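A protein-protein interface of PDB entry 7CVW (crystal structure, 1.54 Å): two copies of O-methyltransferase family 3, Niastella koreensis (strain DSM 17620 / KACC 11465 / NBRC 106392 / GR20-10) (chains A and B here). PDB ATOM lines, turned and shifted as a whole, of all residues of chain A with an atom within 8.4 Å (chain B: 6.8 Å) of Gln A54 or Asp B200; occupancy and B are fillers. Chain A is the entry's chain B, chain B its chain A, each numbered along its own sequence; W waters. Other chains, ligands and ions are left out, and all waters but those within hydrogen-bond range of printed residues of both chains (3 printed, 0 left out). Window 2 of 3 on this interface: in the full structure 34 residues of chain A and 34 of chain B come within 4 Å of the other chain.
No position is printed for both chains.
The side-chain amino group of Lys A47 lies within hydrogen-bond range of the backbone carbonyl oxygen of Leu A17, at 2.9 Å. The backbone carbonyl oxygen (O) of Leu B217 sits at hydrogen-bond distance from the backbone NH (N) of Thr B202, 2.9 Å away. O of Asp B200 is in hydrogen-bond range of N of Ile B219 (2.8 Å).
Water W3 lies within hydrogen-bond range of the side-chain carboxylate (OD2) of Asp B200 (2.7 Å), the backbone carbonyl oxygen (O) of Ile B219 (2.9 Å) and the side-chain amide nitrogen (NE2) of Gln A54 (3.2 Å). Water W1 bridges the side-chain hydroxyl of Thr B202 (2.7 Å) and the backbone carbonyl oxygen of Leu A17 (2.9 Å). Water W2 bridges the backbone NH (N) of Ala B201 (2.9 Å) and the side-chain amino group (NZ) of Lys A47 (3.2 Å).
Among the printed residues, pairs that only touch across the chains: Leu A17 with Leu B193 (3.8 Å), Leu A17 with Ala B201 (3.6 Å), Leu A17 with Thr B202 (3.8 Å), Lys A47 with Thr B202 (3.9 Å), Phe A48 with Leu B217 (3.95 Å), Leu A51 with Asp B200 (3.6 Å), Leu A51 with Ala B201 (3.8 Å), Leu A51 with Thr B202 (3.5 Å), Leu A51 with Ile B219 (3.3 Å), Gln A54 with Ile B219 (3.8 Å) and Leu A55 with Ile B219 (3.7 Å).
Of the 14 printed residues of chain B, 6 touch a printed residue of chain A. Printed residues of chain B that touch a printed residue of chain A: Leu B193, Asp B200, Ala B201, Thr B202, Leu B217 and Ile B219. Of the 23 printed residues of chain A, 6 touch a printed residue of chain B. Among the printed residues, no Asp or Glu carboxylate lies within 4 Å of a Lys or Arg side-chain nitrogen of the other chain.
Of chain B, only Asp B200 (3.1 Å) and Ile B219 (3.8 Å) come within 4 Å of Gln A54. Of chain A, only Leu A51 (3.6 Å) and Gln A54 (3.1 Å) come within 4 Å of Asp B200. Printed residues of chain B within 4 Å of Leu A51: Asp B200 (3.6 Å), Ala B201 (3.8 Å), Thr B202 (3.5 Å) and Ile B219 (3.3 Å). Printed residues of chain A within 4 Å of Leu B217: Phe A48 (3.95 Å). Val B220 touches none of the printed residues of chain A. The nearest residue of chain A that does not touch Asp B200 is Lys A47 (4.6 Å). The nearest printed residue of chain B that does not touch Leu A55 is Gly B159 (4.5 Å).
O of Ala B201 sits at hydrogen-bond distance from NZ of Lys A47 (3.0 Å). The side-chain carboxylate (OD2) of Asp B200 lies within hydrogen-bond range of the side-chain amide nitrogen (NE2) of Gln A54, 3.1 Å away.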
ATOM      1  N   LEU A  17     -37.054 -25.892   5.970  1.00  0.00           N
ATOM      2  CA  LEU A  17     -35.609 -26.182   6.194  1.00  0.00           C
ATOM      3  C   LEU A  17     -35.036 -27.194   5.189  1.00  0.00           C
ATOM      4  O   LEU A  17     -33.876 -27.650   5.419  1.00  0.00           O
ATOM      5  CB  LEU A  17     -35.414 -26.694   7.632  1.00  0.00           C
ATOM      6  CG  LEU A  17     -35.714 -25.682   8.741  1.00  0.00           C
ATOM      7  CD1 LEU A  17     -35.771 -26.409  10.077  1.00  0.00           C
ATOM      8  CD2 LEU A  17     -34.680 -24.558   8.752  1.00  0.00           C
ATOM      9  N   GLY A  46     -31.153 -35.566   3.724  1.00  0.00           N
ATOM     10  CA  GLY A  46     -30.011 -34.928   3.046  1.00  0.00           C
ATOM     11  C   GLY A  46     -29.506 -33.750   3.842  1.00  0.00           C
ATOM     12  O   GLY A  46     -28.300 -33.640   4.060  1.00  0.00           O
ATOM     13  N   LYS A  47     -30.423 -32.927   4.332  1.00  0.00           N
ATOM     14  CA  LYS A  47     -30.037 -31.750   5.138  1.00  0.00           C
ATOM     15  C   LYS A  47     -29.335 -32.248   6.409  1.00  0.00           C
ATOM     16  O   LYS A  47     -28.312 -31.700   6.810  1.00  0.00           O
ATOM     17  CB  LYS A  47     -31.257 -30.881   5.433  1.00  0.00           C
ATOM     18  CG  LYS A  47     -30.922 -29.620   6.211  1.00  0.00           C
ATOM     19  CD  LYS A  47     -30.052 -28.611   5.432  1.00  0.00           C
ATOM     20  CE  LYS A  47     -29.995 -27.241   6.084  1.00  0.00           C
ATOM     21  NZ  LYS A  47     -31.244 -26.482   5.862  1.00  0.00           N
ATOM     22  N   PHE A  48     -29.899 -33.258   7.053  1.00  0.00           N
ATOM     23  CA  PHE A  48     -29.302 -33.865   8.258  1.00  0.00           C
ATOM     24  C   PHE A  48     -27.877 -34.366   7.978  1.00  0.00           C
ATOM     25  O   PHE A  48     -26.957 -34.039   8.756  1.00  0.00           O
ATOM     26  CB  PHE A  48     -30.224 -34.958   8.778  1.00  0.00           C
ATOM     27  CG  PHE A  48     -29.720 -35.667  10.013  1.00  0.00           C
ATOM     28  CD1 PHE A  48     -29.256 -34.963  11.118  1.00  0.00           C
ATOM     29  CD2 PHE A  48     -29.729 -37.054  10.075  1.00  0.00           C
ATOM     30  CE1 PHE A  48     -28.816 -35.636  12.254  1.00  0.00           C
ATOM     31  CE2 PHE A  48     -29.310 -37.724  11.220  1.00  0.00           C
ATOM     32  CZ  PHE A  48     -28.824 -37.019  12.294  1.00  0.00           C
ATOM     33  N   LEU A  49     -27.643 -35.115   6.884  1.00  0.00           N
ATOM     34  CA  LEU A  49     -26.270 -35.585   6.550  1.00  0.00           C
ATOM     35  C   LEU A  49     -25.334 -34.394   6.297  1.00  0.00           C
ATOM     36  O   LEU A  49     -24.155 -34.448   6.729  1.00  0.00           O
ATOM     37  CB  LEU A  49     -26.291 -36.481   5.308  1.00  0.00           C
ATOM     38  CG  LEU A  49     -27.042 -37.807   5.461  1.00  0.00           C
ATOM     39  CD1 LEU A  49     -27.045 -38.502   4.112  1.00  0.00           C
ATOM     40  CD2 LEU A  49     -26.412 -38.725   6.506  1.00  0.00           C
ATOM     41  N   GLN A  50     -25.839 -33.329   5.678  1.00  0.00           N
ATOM     42  CA  GLN A  50     -25.044 -32.100   5.428  1.00  0.00           C
ATOM     43  C   GLN A  50     -24.624 -31.507   6.779  1.00  0.00           C
ATOM     44  O   GLN A  50     -23.463 -31.137   6.963  1.00  0.00           O
ATOM     45  CB  GLN A  50     -25.830 -31.094   4.605  1.00  0.00           C
ATOM     46  CG  GLN A  50     -24.982 -29.913   4.188  1.00  0.00           C
ATOM     47  CD  GLN A  50     -25.788 -29.008   3.297  1.00  0.00           C
ATOM     48  OE1 GLN A  50     -26.549 -28.172   3.780  1.00  0.00           O
ATOM     49  NE2 GLN A  50     -25.696 -29.243   1.991  1.00  0.00           N
ATOM     50  N   LEU A  51     -25.545 -31.448   7.723  1.00  0.00           N
ATOM     51  CA  LEU A  51     -25.264 -30.845   9.037  1.00  0.00           C
ATOM     52  C   LEU A  51     -24.255 -31.725   9.768  1.00  0.00           C
ATOM     53  O   LEU A  51     -23.350 -31.177  10.429  1.00  0.00           O
ATOM     54  CB  LEU A  51     -26.560 -30.691   9.829  1.00  0.00           C
ATOM     55  CG  LEU A  51     -27.562 -29.697   9.246  1.00  0.00           C
ATOM     56  CD1 LEU A  51     -28.880 -29.774   9.990  1.00  0.00           C
ATOM     57  CD2 LEU A  51     -27.006 -28.299   9.259  1.00  0.00           C
ATOM     58  N   LEU A  52     -24.411 -33.037   9.703  1.00  0.00           N
ATOM     59  CA  LEU A  52     -23.431 -33.939  10.354  1.00  0.00           C
ATOM     60  C   LEU A  52     -22.057 -33.695   9.749  1.00  0.00           C
ATOM     61  O   LEU A  52     -21.084 -33.607  10.511  1.00  0.00           O
ATOM     62  CB  LEU A  52     -23.865 -35.393  10.195  1.00  0.00           C
ATOM     63  CG  LEU A  52     -25.101 -35.763  10.995  1.00  0.00           C
ATOM     64  CD1 LEU A  52     -25.576 -37.143  10.568  1.00  0.00           C
ATOM     65  CD2 LEU A  52     -24.827 -35.701  12.482  1.00  0.00           C
ATOM     66  N   ALA A  53     -21.964 -33.561   8.433  1.00  0.00           N
ATOM     67  CA  ALA A  53     -20.672 -33.275   7.773  1.00  0.00           C
ATOM     68  C   ALA A  53     -20.101 -31.952   8.305  1.00  0.00           C
ATOM     69  O   ALA A  53     -18.894 -31.888   8.550  1.00  0.00           O
ATOM     70  CB  ALA A  53     -20.854 -33.249   6.277  1.00  0.00           C
ATOM     71  N   GLN A  54     -20.929 -30.924   8.499  1.00  0.00           N
ATOM     72  CA  GLN A  54     -20.462 -29.624   9.060  1.00  0.00           C
ATOM     73  C   GLN A  54     -19.980 -29.815  10.497  1.00  0.00           C
ATOM     74  O   GLN A  54     -18.938 -29.233  10.844  1.00  0.00           O
ATOM     75  CB  GLN A  54     -21.573 -28.581   9.000  1.00  0.00           C
ATOM     76  CG  GLN A  54     -21.945 -28.188   7.591  1.00  0.00           C
ATOM     77  CD  GLN A  54     -23.084 -27.205   7.579  1.00  0.00           C
ATOM     78  OE1 GLN A  54     -24.194 -27.528   7.161  1.00  0.00           O
ATOM     79  NE2 GLN A  54     -22.842 -26.028   8.125  1.00  0.00           N
ATOM     80  N   LEU A  55     -20.683 -30.623  11.308  1.00  0.00           N
ATOM     81  CA  LEU A  55     -20.289 -30.872  12.720  1.00  0.00           C
ATOM     82  C   LEU A  55     -18.923 -31.565  12.755  1.00  0.00           C
ATOM     83  O   LEU A  55     -18.127 -31.224  13.639  1.00  0.00           O
ATOM     84  CB  LEU A  55     -21.322 -31.735  13.448  1.00  0.00           C
ATOM     85  CG  LEU A  55     -22.566 -31.001  13.927  1.00  0.00           C
ATOM     86  CD1 LEU A  55     -23.496 -31.969  14.641  1.00  0.00           C
ATOM     87  CD2 LEU A  55     -22.216 -29.816  14.830  1.00  0.00           C
ATOM     88  N   CYS A  56     -18.660 -32.473  11.815  1.00  0.00           N
ATOM     89  CA  CYS A  56     -17.370 -33.209  11.667  1.00  0.00           C
ATOM     90  C   CYS A  56     -16.251 -32.291  11.150  1.00  0.00           C
ATOM     91  O   CYS A  56     -15.115 -32.805  11.035  1.00  0.00           O
ATOM     92  CB  CYS A  56     -17.497 -34.371  10.679  1.00  0.00           C
ATOM     93  SG  CYS A  56     -18.537 -35.709  11.290  1.00  0.00           S
ATOM     94  N   GLN A  57     -16.570 -31.055  10.747  1.00  0.00           N
ATOM     95  CA  GLN A  57     -15.692 -30.153   9.955  1.00  0.00           C
ATOM     96  C   GLN A  57     -15.076 -30.969   8.806  1.00  0.00           C
ATOM     97  O   GLN A  57     -13.821 -30.983   8.624  1.00  0.00           O
ATOM     98  CB  GLN A  57     -14.637 -29.523  10.861  1.00  0.00           C
ATOM     99  CG  GLN A  57     -15.236 -28.525  11.840  1.00  0.00           C
ATOM    100  CD  GLN A  57     -14.162 -27.892  12.681  1.00  0.00           C
ATOM    101  OE1 GLN A  57     -13.549 -28.546  13.519  1.00  0.00           O
ATOM    102  NE2 GLN A  57     -13.914 -26.615  12.451  1.00  0.00           N
ATOM    103  N   ALA A  58     -15.925 -31.703   8.089  1.00  0.00           N
ATOM    104  CA  ALA A  58     -15.466 -32.683   7.088  1.00  0.00           C
ATOM    105  C   ALA A  58     -14.685 -31.989   5.958  1.00  0.00           C
ATOM    106  O   ALA A  58     -15.162 -30.983   5.388  1.00  0.00           O
ATOM    107  CB  ALA A  58     -16.631 -33.488   6.572  1.00  0.00           C
ATOM    108  N   LYS A  59     -13.508 -32.539   5.648  1.00  0.00           N
ATOM    109  CA  LYS A  59     -12.680 -32.192   4.454  1.00  0.00           C
ATOM    110  C   LYS A  59     -12.594 -33.402   3.511  1.00  0.00           C
ATOM    111  O   LYS A  59     -12.315 -33.218   2.327  1.00  0.00           O
ATOM    112  CB  LYS A  59     -11.268 -31.792   4.889  1.00  0.00           C
ATOM    113  CG  LYS A  59     -11.191 -30.877   6.105  1.00  0.00           C
ATOM    114  CD  LYS A  59     -11.459 -29.426   5.792  1.00  0.00           C
ATOM    115  CE  LYS A  59     -11.288 -28.515   6.990  1.00  0.00           C
ATOM    116  NZ  LYS A  59     -11.468 -27.090   6.617  1.00  0.00           N
ATOM    117  N   ILE A  61     -14.712 -37.107   2.747  1.00  0.00           N
ATOM    118  CA  ILE A  61     -15.910 -37.959   3.002  1.00  0.00           C
ATOM    119  C   ILE A  61     -15.842 -39.182   2.097  1.00  0.00           C
ATOM    120  O   ILE A  61     -15.421 -39.049   0.941  1.00  0.00           O
ATOM    121  CB  ILE A  61     -17.196 -37.164   2.760  1.00  0.00           C
ATOM    122  CG1 ILE A  61     -17.291 -35.964   3.709  1.00  0.00           C
ATOM    123  CG2 ILE A  61     -18.408 -38.077   2.878  1.00  0.00           C
ATOM    124  CD1 ILE A  61     -18.462 -35.053   3.440  1.00  0.00           C
ATOM    125  N   TRP A  74     -25.776 -33.466  -1.331  1.00  0.00           N
ATOM    126  CA  TRP A  74     -26.010 -32.875   0.008  1.00  0.00           C
ATOM    127  C   TRP A  74     -24.707 -32.860   0.821  1.00  0.00           C
ATOM    128  O   TRP A  74     -24.381 -31.816   1.441  1.00  0.00           O
ATOM    129  CB  TRP A  74     -27.105 -33.640   0.735  1.00  0.00           C
ATOM    130  CG  TRP A  74     -28.496 -33.206   0.427  1.00  0.00           C
ATOM    131  CD1 TRP A  74     -29.412 -33.915  -0.298  1.00  0.00           C
ATOM    132  CD2 TRP A  74     -29.160 -32.005   0.859  1.00  0.00           C
ATOM    133  NE1 TRP A  74     -30.601 -33.250  -0.319  1.00  0.00           N
ATOM    134  CE2 TRP A  74     -30.485 -32.082   0.378  1.00  0.00           C
ATOM    135  CE3 TRP A  74     -28.796 -30.903   1.640  1.00  0.00           C
ATOM    136  CZ2 TRP A  74     -31.442 -31.093   0.608  1.00  0.00           C
ATOM    137  CZ3 TRP A  74     -29.735 -29.918   1.854  1.00  0.00           C
ATOM    138  CH2 TRP A  74     -31.025 -29.995   1.325  1.00  0.00           C
ATOM    139  N   MET A  75     -23.996 -33.990   0.897  1.00  0.00           N
ATOM    140  CA  MET A  75     -22.780 -34.054   1.746  1.00  0.00           C
ATOM    141  C   MET A  75     -21.641 -33.264   1.116  1.00  0.00           C
ATOM    142  O   MET A  75     -20.943 -32.557   1.843  1.00  0.00           O
ATOM    143  CB  MET A  75     -22.323 -35.487   1.997  1.00  0.00           C
ATOM    144  CG  MET A  75     -23.263 -36.214   2.925  1.00  0.00           C
ATOM    145  SD  MET A  75     -22.723 -37.885   3.299  1.00  0.00           S
ATOM    146  CE  MET A  75     -22.950 -38.697   1.719  1.00  0.00           C
ATOM    147  N   ARG A  77     -21.695 -30.587  -0.548  1.00  0.00           N
ATOM    148  CA  ARG A  77     -21.949 -29.139  -0.351  1.00  0.00           C
ATOM    149  C   ARG A  77     -21.494 -28.664   1.038  1.00  0.00           C
ATOM    150  O   ARG A  77     -21.343 -27.432   1.197  1.00  0.00           O
ATOM    151  CB  ARG A  77     -23.403 -28.806  -0.650  1.00  0.00           C
ATOM    152  CG  ARG A  77     -23.664 -28.769  -2.139  1.00  0.00           C
ATOM    153  CD  ARG A  77     -25.110 -28.585  -2.485  1.00  0.00           C
ATOM    154  NE  ARG A  77     -25.288 -28.291  -3.906  1.00  0.00           N
ATOM    155  CZ  ARG A  77     -26.463 -28.210  -4.509  1.00  0.00           C
ATOM    156  NH1 ARG A  77     -27.567 -28.402  -3.816  1.00  0.00           N
ATOM    157  NH2 ARG A  77     -26.526 -27.941  -5.803  1.00  0.00           N
ATOM    158  N   ALA A  78     -21.170 -29.564   1.960  1.00  0.00           N
ATOM    159  CA  ALA A  78     -20.636 -29.191   3.293  1.00  0.00           C
ATOM    160  C   ALA A  78     -19.119 -28.994   3.193  1.00  0.00           C
ATOM    161  O   ALA A  78     -18.512 -28.435   4.140  1.00  0.00           O
ATOM    162  CB  ALA A  78     -20.968 -30.241   4.324  1.00  0.00           C
ATOM    163  N   LEU A  79     -18.506 -29.496   2.126  1.00  0.00           N
ATOM    164  CA  LEU A  79     -17.028 -29.514   2.004  1.00  0.00           C
ATOM    165  C   LEU A  79     -16.501 -28.110   1.719  1.00  0.00           C
ATOM    166  O   LEU A  79     -17.118 -27.329   1.010  1.00  0.00           O
ATOM    167  CB  LEU A  79     -16.585 -30.447   0.878  1.00  0.00           C
ATOM    168  CG  LEU A  79     -16.836 -31.936   1.095  1.00  0.00           C
ATOM    169  CD1 LEU A  79     -16.550 -32.689  -0.200  1.00  0.00           C
ATOM    170  CD2 LEU A  79     -16.000 -32.473   2.240  1.00  0.00           C
ATOM    171  N   MET A 135     -15.946 -38.340   7.675  1.00  0.00           N
ATOM    172  CA  MET A 135     -17.323 -38.875   7.735  1.00  0.00           C
ATOM    173  C   MET A 135     -17.411 -39.953   6.674  1.00  0.00           C
ATOM    174  O   MET A 135     -16.847 -39.749   5.577  1.00  0.00           O
ATOM    175  CB  MET A 135     -18.347 -37.776   7.459  1.00  0.00           C
ATOM    176  CG  MET A 135     -19.778 -38.262   7.456  1.00  0.00           C
ATOM    177  SD  MET A 135     -20.878 -36.846   7.449  1.00  0.00           S
ATOM    178  CE  MET A 135     -22.456 -37.670   7.255  1.00  0.00           C
ATOM    179  N   LEU A 161     -17.068 -39.873  12.047  1.00  0.00           N
ATOM    180  CA  LEU A 161     -18.496 -40.246  12.120  1.00  0.00           C
ATOM    181  C   LEU A 161     -18.774 -41.250  11.011  1.00  0.00           C
ATOM    182  O   LEU A 161     -18.490 -40.925   9.833  1.00  0.00           O
ATOM    183  CB  LEU A 161     -19.380 -39.012  11.941  1.00  0.00           C
ATOM    184  CG  LEU A 161     -20.880 -39.274  11.895  1.00  0.00           C
ATOM    185  CD1 LEU A 161     -21.363 -39.861  13.205  1.00  0.00           C
ATOM    186  CD2 LEU A 161     -21.632 -37.993  11.529  1.00  0.00           C
ATOM    187  N   GLY B 159     -20.121 -22.524  14.631  1.00  0.00           N
ATOM    188  CA  GLY B 159     -20.049 -23.986  14.768  1.00  0.00           C
ATOM    189  C   GLY B 159     -20.802 -24.520  15.983  1.00  0.00           C
ATOM    190  O   GLY B 159     -20.905 -25.745  16.122  1.00  0.00           O
ATOM    191  N   LEU B 193     -37.144 -20.565  12.894  1.00  0.00           N
ATOM    192  CA  LEU B 193     -35.967 -21.323  12.452  1.00  0.00           C
ATOM    193  C   LEU B 193     -35.912 -21.313  10.918  1.00  0.00           C
ATOM    194  O   LEU B 193     -34.806 -21.089  10.371  1.00  0.00           O
ATOM    195  CB  LEU B 193     -36.068 -22.717  13.083  1.00  0.00           C
ATOM    196  CG  LEU B 193     -34.798 -23.535  13.055  1.00  0.00           C
ATOM    197  CD1 LEU B 193     -33.646 -22.799  13.723  1.00  0.00           C
ATOM    198  CD2 LEU B 193     -35.071 -24.881  13.689  1.00  0.00           C
ATOM    199  N   ASN B 196     -34.441 -18.001   9.788  1.00  0.00           N
ATOM    200  CA  ASN B 196     -33.195 -17.560  10.448  1.00  0.00           C
ATOM    201  C   ASN B 196     -32.015 -17.737   9.495  1.00  0.00           C
ATOM    202  O   ASN B 196     -31.756 -18.882   9.088  1.00  0.00           O
ATOM    203  CB  ASN B 196     -33.009 -18.310  11.766  1.00  0.00           C
ATOM    204  CG  ASN B 196     -31.951 -17.677  12.622  1.00  0.00           C
ATOM    205  OD1 ASN B 196     -30.767 -17.762  12.294  1.00  0.00           O
ATOM    206  ND2 ASN B 196     -32.358 -17.138  13.757  1.00  0.00           N
ATOM    207  N   THR B 197     -31.268 -16.663   9.236  1.00  0.00           N
ATOM    208  CA  THR B 197     -30.100 -16.658   8.327  1.00  0.00           C
ATOM    209  C   THR B 197     -28.804 -16.855   9.115  1.00  0.00           C
ATOM    210  O   THR B 197     -27.766 -16.910   8.448  1.00  0.00           O
ATOM    211  CB  THR B 197     -30.040 -15.353   7.531  1.00  0.00           C
ATOM    212  OG1 THR B 197     -29.949 -14.302   8.482  1.00  0.00           O
ATOM    213  CG2 THR B 197     -31.268 -15.150   6.676  1.00  0.00           C
ATOM    214  N   ALA B 198     -28.835 -16.958  10.454  1.00  0.00           N
ATOM    215  CA  ALA B 198     -27.616 -17.091  11.288  1.00  0.00           C
ATOM    216  C   ALA B 198     -27.242 -18.569  11.439  1.00  0.00           C
ATOM    217  O   ALA B 198     -26.186 -18.840  11.993  1.00  0.00           O
ATOM    218  CB  ALA B 198     -27.835 -16.464  12.643  1.00  0.00           C
ATOM    219  N   VAL B 199     -28.126 -19.495  11.060  1.00  0.00           N
ATOM    220  CA  VAL B 199     -27.892 -20.946  11.304  1.00  0.00           C
ATOM    221  C   VAL B 199     -28.245 -21.753  10.053  1.00  0.00           C
ATOM    222  O   VAL B 199     -29.055 -21.273   9.215  1.00  0.00           O
ATOM    223  CB  VAL B 199     -28.703 -21.500  12.493  1.00  0.00           C
ATOM    224  CG1 VAL B 199     -28.398 -20.773  13.787  1.00  0.00           C
ATOM    225  CG2 VAL B 199     -30.202 -21.527  12.214  1.00  0.00           C
ATOM    226  N   ASP B 200     -27.668 -22.957   9.977  1.00  0.00           N
ATOM    227  CA  ASP B 200     -28.094 -24.067   9.091  1.00  0.00           C
ATOM    228  C   ASP B 200     -28.834 -25.073   9.968  1.00  0.00           C
ATOM    229  O   ASP B 200     -28.296 -25.435  11.042  1.00  0.00           O
ATOM    230  CB  ASP B 200     -26.887 -24.714   8.423  1.00  0.00           C
ATOM    231  CG  ASP B 200     -26.129 -23.749   7.518  1.00  0.00           C
ATOM    232  OD1 ASP B 200     -26.796 -23.046   6.755  1.00  0.00           O
ATOM    233  OD2 ASP B 200     -24.884 -23.711   7.585  1.00  0.00           O
ATOM    234  N   ALA B 201     -30.045 -25.470   9.602  1.00  0.00           N
ATOM    235  CA  ALA B 201     -30.871 -26.257  10.539  1.00  0.00           C
ATOM    236  C   ALA B 201     -31.747 -27.286   9.837  1.00  0.00           C
ATOM    237  O   ALA B 201     -32.034 -27.159   8.629  1.00  0.00           O
ATOM    238  CB  ALA B 201     -31.730 -25.325  11.359  1.00  0.00           C
ATOM    239  N   THR B 202     -32.202 -28.265  10.610  1.00  0.00           N
ATOM    240  CA  THR B 202     -33.224 -29.240  10.190  1.00  0.00           C
ATOM    241  C   THR B 202     -34.090 -29.531  11.403  1.00  0.00           C
ATOM    242  O   THR B 202     -33.767 -29.098  12.502  1.00  0.00           O
ATOM    243  CB  THR B 202     -32.608 -30.522   9.605  1.00  0.00           C
ATOM    244  OG1 THR B 202     -33.668 -31.242   8.953  1.00  0.00           O
ATOM    245  CG2 THR B 202     -31.943 -31.386  10.656  1.00  0.00           C
ATOM    246  N   LEU B 217     -32.271 -29.229  15.059  1.00  0.00           N
ATOM    247  CA  LEU B 217     -30.798 -29.187  15.144  1.00  0.00           C
ATOM    248  C   LEU B 217     -30.340 -28.005  14.306  1.00  0.00           C
ATOM    249  O   LEU B 217     -30.739 -27.933  13.138  1.00  0.00           O
ATOM    250  CB  LEU B 217     -30.196 -30.483  14.591  1.00  0.00           C
ATOM    251  CG  LEU B 217     -30.046 -31.645  15.572  1.00  0.00           C
ATOM    252  CD1 LEU B 217     -31.379 -32.152  16.046  1.00  0.00           C
ATOM    253  CD2 LEU B 217     -29.216 -32.774  14.953  1.00  0.00           C
ATOM    254  N   ALA B 218     -29.528 -27.127  14.878  1.00  0.00           N
ATOM    255  CA  ALA B 218     -29.048 -25.922  14.170  1.00  0.00           C
ATOM    256  C   ALA B 218     -27.559 -25.737  14.433  1.00  0.00           C
ATOM    257  O   ALA B 218     -27.126 -25.859  15.589  1.00  0.00           O
ATOM    258  CB  ALA B 218     -29.858 -24.736  14.618  1.00  0.00           C
ATOM    259  N   ILE B 219     -26.804 -25.404  13.391  1.00  0.00           N
ATOM    260  CA  ILE B 219     -25.369 -25.061  13.519  1.00  0.00           C
ATOM    261  C   ILE B 219     -25.205 -23.582  13.212  1.00  0.00           C
ATOM    262  O   ILE B 219     -25.632 -23.115  12.147  1.00  0.00           O
ATOM    263  CB  ILE B 219     -24.484 -25.944  12.638  1.00  0.00           C
ATOM    264  CG1 ILE B 219     -24.779 -27.416  12.875  1.00  0.00           C
ATOM    265  CG2 ILE B 219     -23.027 -25.604  12.897  1.00  0.00           C
ATOM    266  CD1 ILE B 219     -24.079 -28.304  11.899  1.00  0.00           C
ATOM    267  N   VAL B 220     -24.584 -22.862  14.147  1.00  0.00           N
ATOM    268  CA  VAL B 220     -24.357 -21.399  14.035  1.00  0.00           C
ATOM    269  C   VAL B 220     -23.296 -21.121  12.949  1.00  0.00           C
ATOM    270  O   VAL B 220     -22.215 -21.712  12.992  1.00  0.00           O
ATOM    271  CB  VAL B 220     -23.987 -20.795  15.399  1.00  0.00           C
ATOM    272  CG1 VAL B 220     -23.715 -19.307  15.267  1.00  0.00           C
ATOM    273  CG2 VAL B 220     -25.097 -21.042  16.410  1.00  0.00           C
ATOM    274  N   LYS B 221     -23.616 -20.241  12.002  1.00  0.00           N
ATOM    275  CA  LYS B 221     -22.715 -19.916  10.854  1.00  0.00           C
ATOM    276  C   LYS B 221     -21.649 -18.916  11.326  1.00  0.00           C
ATOM    277  O   LYS B 221     -22.008 -18.036  12.126  1.00  0.00           O
ATOM    278  CB  LYS B 221     -23.564 -19.422   9.675  1.00  0.00           C
ATOM    279  CG  LYS B 221     -24.615 -20.433   9.237  1.00  0.00           C
ATOM    280  CD  LYS B 221     -25.417 -20.155   7.989  1.00  0.00           C
ATOM    281  CE  LYS B 221     -25.504 -18.718   7.563  1.00  0.00           C
ATOM    282  NZ  LYS B 221     -26.577 -18.566   6.548  1.00  0.00           N
HETATM  283  O   HOH W   1     -34.483 -30.295   6.572  1.00  0.00           O
HETATM  284  O   HOH W   2     -31.263 -23.811   7.551  1.00  0.00           O
HETATM  285  O   HOH W   3     -23.728 -23.576  10.001  1.00  0.00           O
